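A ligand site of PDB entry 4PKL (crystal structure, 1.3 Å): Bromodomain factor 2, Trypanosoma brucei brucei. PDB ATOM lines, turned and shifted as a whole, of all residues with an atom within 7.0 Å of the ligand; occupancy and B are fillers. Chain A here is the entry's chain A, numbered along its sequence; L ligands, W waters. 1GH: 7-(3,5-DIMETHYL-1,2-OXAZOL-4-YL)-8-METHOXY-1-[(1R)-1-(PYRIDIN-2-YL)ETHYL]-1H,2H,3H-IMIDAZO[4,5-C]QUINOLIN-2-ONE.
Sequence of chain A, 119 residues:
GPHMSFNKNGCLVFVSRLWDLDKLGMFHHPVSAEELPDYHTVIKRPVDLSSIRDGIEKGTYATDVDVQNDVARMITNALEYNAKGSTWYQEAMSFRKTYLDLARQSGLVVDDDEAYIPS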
ATOM      1  N   ASP A  22      25.194  14.918  -5.960  1.00  0.00           N
ATOM      2  CA  ASP A  22      25.621  13.804  -5.107  1.00  0.00           C
ATOM      3  C   ASP A  22      26.431  14.321  -3.924  1.00  0.00           C
ATOM      4  O   ASP A  22      27.663  14.267  -3.916  1.00  0.00           O
ATOM      5  CB  ASP A  22      26.459  12.833  -5.925  1.00  0.00           C
ATOM      6  CG  ASP A  22      27.017  11.675  -5.120  1.00  0.00           C
ATOM      7  OD1 ASP A  22      26.584  11.423  -3.961  1.00  0.00           O
ATOM      8  OD2 ASP A  22      27.921  11.023  -5.659  1.00  0.00           O
ATOM      9  N   LEU A  24      26.806  13.267  -0.912  1.00  0.00           N
ATOM     10  CA  LEU A  24      27.568  12.274  -0.194  1.00  0.00           C
ATOM     11  C   LEU A  24      28.794  11.822  -0.981  1.00  0.00           C
ATOM     12  O   LEU A  24      29.691  11.199  -0.416  1.00  0.00           O
ATOM     13  CB  LEU A  24      26.715  11.048   0.140  1.00  0.00           C
ATOM     14  CG  LEU A  24      25.660  11.259   1.221  1.00  0.00           C
ATOM     15  CD1 LEU A  24      24.641  10.121   1.189  1.00  0.00           C
ATOM     16  CD2 LEU A  24      26.331  11.302   2.583  1.00  0.00           C
ATOM     17  N   GLY A  25      28.864  12.146  -2.261  1.00  0.00           N
ATOM     18  CA  GLY A  25      29.917  11.618  -3.122  1.00  0.00           C
ATOM     19  C   GLY A  25      29.818  10.102  -3.268  1.00  0.00           C
ATOM     20  O   GLY A  25      30.819   9.445  -3.594  1.00  0.00           O
ATOM     21  N   MET A  26      28.626   9.556  -3.049  1.00  0.00           N
ATOM     22  CA  MET A  26      28.443   8.111  -3.028  1.00  0.00           C
ATOM     23  C   MET A  26      28.470   7.488  -4.428  1.00  0.00           C
ATOM     24  O   MET A  26      28.607   6.281  -4.564  1.00  0.00           O
ATOM     25  CB  MET A  26      27.117   7.743  -2.335  1.00  0.00           C
ATOM     26  CG  MET A  26      25.874   8.275  -3.032  1.00  0.00           C
ATOM     27  SD  MET A  26      24.326   7.877  -2.177  1.00  0.00           S
ATOM     28  CE  MET A  26      24.165   6.149  -2.570  1.00  0.00           C
ATOM     29  N   PHE A  27      28.344   8.335  -5.448  1.00  0.00           N
ATOM     30  CA  PHE A  27      28.350   7.909  -6.849  1.00  0.00           C
ATOM     31  C   PHE A  27      29.614   8.332  -7.578  1.00  0.00           C
ATOM     32  O   PHE A  27      29.777   8.035  -8.757  1.00  0.00           O
ATOM     33  CB  PHE A  27      27.135   8.475  -7.601  1.00  0.00           C
ATOM     34  CG  PHE A  27      25.802   8.001  -7.091  1.00  0.00           C
ATOM     35  CD1 PHE A  27      25.458   6.662  -7.144  1.00  0.00           C
ATOM     36  CD2 PHE A  27      24.874   8.908  -6.586  1.00  0.00           C
ATOM     37  CE1 PHE A  27      24.194   6.231  -6.720  1.00  0.00           C
ATOM     38  CE2 PHE A  27      23.630   8.482  -6.148  1.00  0.00           C
ATOM     39  CZ  PHE A  27      23.297   7.133  -6.221  1.00  0.00           C
ATOM     40  N   HIS A  28      30.509   9.041  -6.899  1.00  0.00           N
ATOM     41  CA  HIS A  28      31.628   9.676  -7.604  1.00  0.00           C
ATOM     42  C   HIS A  28      32.672   8.706  -8.140  1.00  0.00           C
ATOM     43  O   HIS A  28      33.246   8.965  -9.213  1.00  0.00           O
ATOM     44  CB  HIS A  28      32.309  10.703  -6.713  1.00  0.00           C
ATOM     45  CG  HIS A  28      31.537  11.968  -6.528  1.00  0.00           C
ATOM     46  ND1 HIS A  28      31.982  12.989  -5.706  1.00  0.00           N
ATOM     47  CD2 HIS A  28      30.374  12.404  -7.070  1.00  0.00           C
ATOM     48  CE1 HIS A  28      31.117  13.984  -5.752  1.00  0.00           C
ATOM     49  NE2 HIS A  28      30.121  13.656  -6.557  1.00  0.00           N
ATOM     50  N   HIS A  29      32.955   7.622  -7.423  1.00  0.00           N
ATOM     51  CA  HIS A  29      34.112   6.774  -7.714  1.00  0.00           C
ATOM     52  C   HIS A  29      33.784   5.299  -7.621  1.00  0.00           C
ATOM     53  O   HIS A  29      32.890   4.899  -6.870  1.00  0.00           O
ATOM     54  CB  HIS A  29      35.266   7.065  -6.748  1.00  0.00           C
ATOM     55  CG  HIS A  29      35.677   8.499  -6.711  1.00  0.00           C
ATOM     56  ND1 HIS A  29      36.402   9.094  -7.721  1.00  0.00           N
ATOM     57  CD2 HIS A  29      35.468   9.460  -5.776  1.00  0.00           C
ATOM     58  CE1 HIS A  29      36.606  10.369  -7.419  1.00  0.00           C
ATOM     59  NE2 HIS A  29      36.055  10.613  -6.247  1.00  0.00           N
ATOM     60  N   PRO A  30      34.570   4.462  -8.323  1.00  0.00           N
ATOM     61  CA  PRO A  30      34.438   3.027  -8.072  1.00  0.00           C
ATOM     62  C   PRO A  30      34.816   2.737  -6.635  1.00  0.00           C
ATOM     63  O   PRO A  30      35.649   3.426  -6.043  1.00  0.00           O
ATOM     64  CB  PRO A  30      35.428   2.393  -9.049  1.00  0.00           C
ATOM     65  CG  PRO A  30      36.370   3.487  -9.415  1.00  0.00           C
ATOM     66  CD  PRO A  30      35.622   4.770  -9.309  1.00  0.00           C
ATOM     67  N   VAL A  31      34.205   1.698  -6.079  1.00  0.00           N
ATOM     68  CA  VAL A  31      34.437   1.295  -4.703  1.00  0.00           C
ATOM     69  C   VAL A  31      35.650   0.389  -4.643  1.00  0.00           C
ATOM     70  O   VAL A  31      35.726  -0.604  -5.361  1.00  0.00           O
ATOM     71  CB  VAL A  31      33.205   0.583  -4.127  1.00  0.00           C
ATOM     72  CG1 VAL A  31      33.481   0.066  -2.720  1.00  0.00           C
ATOM     73  CG2 VAL A  31      32.038   1.533  -4.110  1.00  0.00           C
ATOM     74  N   SER A  32      36.591   0.747  -3.778  1.00  0.00           N
ATOM     75  CA  SER A  32      37.789  -0.047  -3.556  1.00  0.00           C
ATOM     76  C   SER A  32      37.445  -1.244  -2.670  1.00  0.00           C
ATOM     77  O   SER A  32      36.744  -1.096  -1.670  1.00  0.00           O
ATOM     78  CB  SER A  32      38.882   0.799  -2.909  1.00  0.00           C
ATOM     79  OG  SER A  32      39.714   0.025  -2.075  1.00  0.00           O
ATOM     80  N   GLU A  34      39.419  -2.920  -0.864  1.00  0.00           N
ATOM     81  CA  GLU A  34      40.112  -2.848   0.412  1.00  0.00           C
ATOM     82  C   GLU A  34      39.335  -1.947   1.367  1.00  0.00           C
ATOM     83  O   GLU A  34      39.309  -2.185   2.572  1.00  0.00           O
ATOM     84  CB  GLU A  34      41.546  -2.363   0.220  1.00  0.00           C
ATOM     85  CG  GLU A  34      42.259  -2.035   1.541  1.00  0.00           C
ATOM     86  CD  GLU A  34      43.704  -1.635   1.360  1.00  0.00           C
ATOM     87  OE1 GLU A  34      44.060  -1.156   0.260  1.00  0.00           O
ATOM     88  OE2 GLU A  34      44.494  -1.797   2.308  1.00  0.00           O
ATOM     89  N   GLU A  35      38.707  -0.909   0.840  1.00  0.00           N
ATOM     90  CA  GLU A  35      38.008   0.034   1.704  1.00  0.00           C
ATOM     91  C   GLU A  35      36.627  -0.493   2.136  1.00  0.00           C
ATOM     92  O   GLU A  35      36.233  -0.342   3.293  1.00  0.00           O
ATOM     93  CB  GLU A  35      37.850   1.381   1.011  1.00  0.00           C
ATOM     94  CG  GLU A  35      37.393   2.473   1.938  1.00  0.00           C
ATOM     95  CD  GLU A  35      37.497   3.852   1.318  1.00  0.00           C
ATOM     96  OE1 GLU A  35      37.632   3.956   0.080  1.00  0.00           O
ATOM     97  OE2 GLU A  35      37.449   4.833   2.088  1.00  0.00           O
ATOM     98  N   LEU A  36      35.910  -1.122   1.214  1.00  0.00           N
ATOM     99  CA  LEU A  36      34.575  -1.615   1.500  1.00  0.00           C
ATOM    100  C   LEU A  36      34.401  -3.018   0.921  1.00  0.00           C
ATOM    101  O   LEU A  36      33.792  -3.195  -0.134  1.00  0.00           O
ATOM    102  CB  LEU A  36      33.535  -0.633   0.943  1.00  0.00           C
ATOM    103  CG  LEU A  36      32.103  -0.665   1.468  1.00  0.00           C
ATOM    104  CD1 LEU A  36      32.004  -0.392   2.968  1.00  0.00           C
ATOM    105  CD2 LEU A  36      31.246   0.321   0.684  1.00  0.00           C
ATOM    106  N   PRO A  37      34.972  -4.036   1.588  1.00  0.00           N
ATOM    107  CA  PRO A  37      35.117  -5.386   1.019  1.00  0.00           C
ATOM    108  C   PRO A  37      33.812  -6.121   0.676  1.00  0.00           C
ATOM    109  O   PRO A  37      33.835  -6.982  -0.193  1.00  0.00           O
ATOM    110  CB  PRO A  37      35.870  -6.156   2.119  1.00  0.00           C
ATOM    111  CG  PRO A  37      36.509  -5.114   2.955  1.00  0.00           C
ATOM    112  CD  PRO A  37      35.595  -3.930   2.920  1.00  0.00           C
ATOM    113  N   TYR A  39      31.127  -4.852  -0.668  1.00  0.00           N
ATOM    114  CA  TYR A  39      30.393  -4.209  -1.760  1.00  0.00           C
ATOM    115  C   TYR A  39      30.352  -5.088  -3.005  1.00  0.00           C
ATOM    116  O   TYR A  39      29.291  -5.284  -3.593  1.00  0.00           O
ATOM    117  CB  TYR A  39      31.002  -2.836  -2.077  1.00  0.00           C
ATOM    118  CG  TYR A  39      30.198  -2.051  -3.088  1.00  0.00           C
ATOM    119  CD1 TYR A  39      30.518  -2.101  -4.449  1.00  0.00           C
ATOM    120  CD2 TYR A  39      29.123  -1.269  -2.705  1.00  0.00           C
ATOM    121  CE1 TYR A  39      29.788  -1.400  -5.379  1.00  0.00           C
ATOM    122  CE2 TYR A  39      28.379  -0.547  -3.622  1.00  0.00           C
ATOM    123  CZ  TYR A  39      28.705  -0.620  -4.969  1.00  0.00           C
ATOM    124  OH  TYR A  39      27.977   0.091  -5.898  1.00  0.00           O
ATOM    125  N   ALA A  78      22.778   1.337  -5.841  1.00  0.00           N
ATOM    126  CA  ALA A  78      22.854   1.991  -4.550  1.00  0.00           C
ATOM    127  C   ALA A  78      21.640   1.674  -3.685  1.00  0.00           C
ATOM    128  O   ALA A  78      21.765   1.594  -2.458  1.00  0.00           O
ATOM    129  CB  ALA A  78      23.003   3.486  -4.738  1.00  0.00           C
ATOM    130  N   TYR A  81      22.456  -1.893  -2.365  1.00  0.00           N
ATOM    131  CA  TYR A  81      23.522  -2.009  -1.383  1.00  0.00           C
ATOM    132  C   TYR A  81      23.148  -1.345  -0.052  1.00  0.00           C
ATOM    133  O   TYR A  81      23.399  -1.901   1.011  1.00  0.00           O
ATOM    134  CB  TYR A  81      24.838  -1.400  -1.900  1.00  0.00           C
ATOM    135  CG  TYR A  81      25.910  -1.496  -0.848  1.00  0.00           C
ATOM    136  CD1 TYR A  81      26.485  -2.717  -0.555  1.00  0.00           C
ATOM    137  CD2 TYR A  81      26.305  -0.384  -0.107  1.00  0.00           C
ATOM    138  CE1 TYR A  81      27.426  -2.846   0.434  1.00  0.00           C
ATOM    139  CE2 TYR A  81      27.262  -0.505   0.887  1.00  0.00           C
ATOM    140  CZ  TYR A  81      27.822  -1.749   1.137  1.00  0.00           C
ATOM    141  OH  TYR A  81      28.769  -1.898   2.118  1.00  0.00           O
ATOM    142  N   ASN A  82      22.581  -0.156  -0.124  1.00  0.00           N
ATOM    143  CA  ASN A  82      22.225   0.587   1.065  1.00  0.00           C
ATOM    144  C   ASN A  82      20.872   0.180   1.635  1.00  0.00           C
ATOM    145  O   ASN A  82      20.018  -0.357   0.926  1.00  0.00           O
ATOM    146  CB  ASN A  82      22.275   2.075   0.743  1.00  0.00           C
ATOM    147  CG  ASN A  82      23.668   2.526   0.403  1.00  0.00           C
ATOM    148  OD1 ASN A  82      24.524   2.600   1.275  1.00  0.00           O
ATOM    149  ND2 ASN A  82      23.937   2.790  -0.884  1.00  0.00           N
ATOM    150  N   SER A  86      18.342   4.819   4.964  1.00  0.00           N
ATOM    151  CA  SER A  86      19.668   5.360   5.286  1.00  0.00           C
ATOM    152  C   SER A  86      19.867   6.646   4.500  1.00  0.00           C
ATOM    153  O   SER A  86      19.149   6.931   3.540  1.00  0.00           O
ATOM    154  CB  SER A  86      20.773   4.347   4.986  1.00  0.00           C
ATOM    155  OG  SER A  86      21.054   4.286   3.597  1.00  0.00           O
ATOM    156  N   TRP A  88      22.285   7.368   2.518  1.00  0.00           N
ATOM    157  CA  TRP A  88      22.652   6.952   1.165  1.00  0.00           C
ATOM    158  C   TRP A  88      21.416   6.570   0.351  1.00  0.00           C
ATOM    159  O   TRP A  88      21.272   6.960  -0.808  1.00  0.00           O
ATOM    160  CB  TRP A  88      23.599   5.756   1.178  1.00  0.00           C
ATOM    161  CG  TRP A  88      24.976   5.959   1.734  1.00  0.00           C
ATOM    162  CD1 TRP A  88      26.076   6.360   1.044  1.00  0.00           C
ATOM    163  CD2 TRP A  88      25.436   5.680   3.070  1.00  0.00           C
ATOM    164  NE1 TRP A  88      27.178   6.376   1.849  1.00  0.00           N
ATOM    165  CE2 TRP A  88      26.813   5.957   3.108  1.00  0.00           C
ATOM    166  CE3 TRP A  88      24.813   5.231   4.242  1.00  0.00           C
ATOM    167  CZ2 TRP A  88      27.574   5.804   4.248  1.00  0.00           C
ATOM    168  CZ3 TRP A  88      25.580   5.085   5.393  1.00  0.00           C
ATOM    169  CH2 TRP A  88      26.948   5.351   5.375  1.00  0.00           C
ATOM    170  N   TYR A  89      20.539   5.769   0.956  1.00  0.00           N
ATOM    171  CA  TYR A  89      19.339   5.301   0.278  1.00  0.00           C
ATOM    172  C   TYR A  89      18.427   6.487  -0.059  1.00  0.00           C
ATOM    173  O   TYR A  89      17.857   6.547  -1.174  1.00  0.00           O
ATOM    174  CB  TYR A  89      18.610   4.287   1.150  1.00  0.00           C
ATOM    175  CG  TYR A  89      17.471   3.541   0.492  1.00  0.00           C
ATOM    176  CD1 TYR A  89      16.198   4.102   0.411  1.00  0.00           C
ATOM    177  CD2 TYR A  89      17.657   2.257  -0.015  1.00  0.00           C
ATOM    178  CE1 TYR A  89      15.156   3.401  -0.162  1.00  0.00           C
ATOM    179  CE2 TYR A  89      16.621   1.563  -0.578  1.00  0.00           C
ATOM    180  CZ  TYR A  89      15.377   2.129  -0.650  1.00  0.00           C
ATOM    181  OH  TYR A  89      14.332   1.440  -1.231  1.00  0.00           O
HETATM  182  O2  1GH L   1      26.806   3.952  -1.189  1.00  0.00           O
HETATM  183  C13 1GH L   1      27.520   3.759  -0.229  1.00  0.00           C
HETATM  184  N1  1GH L   1      28.883   4.082  -0.139  1.00  0.00           N
HETATM  185  C6  1GH L   1      29.564   4.716  -1.232  1.00  0.00           C
HETATM  186  C8  1GH L   1      30.220   6.024  -0.787  1.00  0.00           C
HETATM  187  N2  1GH L   1      29.636   6.735   0.229  1.00  0.00           N
HETATM  188  C12 1GH L   1      30.194   7.910   0.639  1.00  0.00           C
HETATM  189  C11 1GH L   1      31.356   8.390   0.050  1.00  0.00           C
HETATM  190  C10 1GH L   1      31.931   7.680  -0.961  1.00  0.00           C
HETATM  191  C9  1GH L   1      31.381   6.494  -1.378  1.00  0.00           C
HETATM  192  C7  1GH L   1      30.494   3.795  -1.996  1.00  0.00           C
HETATM  193  N3  1GH L   1      27.119   3.181   0.967  1.00  0.00           N
HETATM  194  C14 1GH L   1      28.252   3.174   1.831  1.00  0.00           C
HETATM  195  C5  1GH L   1      29.350   3.702   1.182  1.00  0.00           C
HETATM  196  C15 1GH L   1      28.342   2.691   3.127  1.00  0.00           C
HETATM  197  N4  1GH L   1      29.528   2.755   3.792  1.00  0.00           N
HETATM  198  C16 1GH L   1      30.648   3.295   3.180  1.00  0.00           C
HETATM  199  C4  1GH L   1      30.588   3.764   1.876  1.00  0.00           C
HETATM  200  C3  1GH L   1      31.761   4.281   1.301  1.00  0.00           C
HETATM  201  C17 1GH L   1      31.849   3.337   3.914  1.00  0.00           C
HETATM  202  C18 1GH L   1      33.001   3.839   3.323  1.00  0.00           C
HETATM  203  C2  1GH L   1      32.947   4.316   2.029  1.00  0.00           C
HETATM  204  O1  1GH L   1      34.205   4.767   1.612  1.00  0.00           O
HETATM  205  C1  1GH L   1      34.291   5.112   0.235  1.00  0.00           C
HETATM  206  C19 1GH L   1      34.202   3.906   4.236  1.00  0.00           C
HETATM  207  C22 1GH L   1      34.777   2.941   5.029  1.00  0.00           C
HETATM  208  C23 1GH L   1      34.417   1.475   5.165  1.00  0.00           C
HETATM  209  O3  1GH L   1      35.795   3.500   5.699  1.00  0.00           O
HETATM  210  N5  1GH L   1      35.883   4.838   5.381  1.00  0.00           N
HETATM  211  C20 1GH L   1      34.906   5.090   4.498  1.00  0.00           C
HETATM  212  C21 1GH L   1      34.727   6.492   3.946  1.00  0.00           C
HETATM  213  O   HOH W   1      37.463   1.505   7.696  1.00  0.00           O
HETATM  214  O   HOH W   2      29.428   2.326   6.496  1.00  0.00           O
HETATM  215  O   HOH W   3      26.956   4.006  -3.900  1.00  0.00           O
HETATM  216  O   HOH W   4      36.907   5.343   8.084  1.00  0.00           O
HETATM  217  O   HOH W   5      32.897  11.511  -0.202  1.00  0.00           O
HETATM  218  O   HOH W   6      33.362   5.100  -3.886  1.00  0.00           O
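The indole nitrogen (NE1) of Trp 88 sits at hydrogen-bond distance from a nitrogen (N2) of the ligand (3.0 Å).
N3 of the ligand is in hydrogen-bond range of OD1 of Asn 82.
ND2 of Asn 82 is in hydrogen-bond range of O of Ala 78 (2.9 Å).
The backbone NH (N) of Gly 25 is in hydrogen-bond range of the side-chain carboxylate (OD1) of Asp 22 (2.9 Å).
The backbone NH of Trp 88 sits close to the side-chain hydroxyl of Ser 86, at 3.5 Å.
The backbone NH (N) of Met 26 is in hydrogen-bond range of the side-chain carboxylate (OD1) of Asp 22 (2.9 Å).
The backbone NH (N) of Glu 35 lies within hydrogen-bond range of the side-chain hydroxyl (OG) of Ser 32.
O1 of the ligand sits close to OE2 of Glu 35 (3.3 Å).
Leu 24 touches the ligand.
O of Gly 25 touches C10 of the ligand, 3.4 Å away.
CA of Met 26 touches C8 of the ligand, at 3.5 Å.
Val 31 touches the ligand.
Leu 36 touches the ligand (CD2 to C4, 3.7 Å).
CE2 of Tyr 81 touches N3 of the ligand (3.7 Å).
Hydrophobic or aromatic side chains that line the ligand: Met 26, Val 31, Leu 36, Tyr 81 and Trp 88.
Nine residues have an atom within 4 Å of the ligand: Leu 24, Gly 25, Met 26, Val 31, Glu 35, Leu 36, Tyr 81, Asn 82 and Trp 88.
The nearest printed residue that does not touch the ligand is Tyr 39 (5.1 Å).
Water W3 lies within hydrogen-bond range of O2 of the ligand and O of Met 26.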
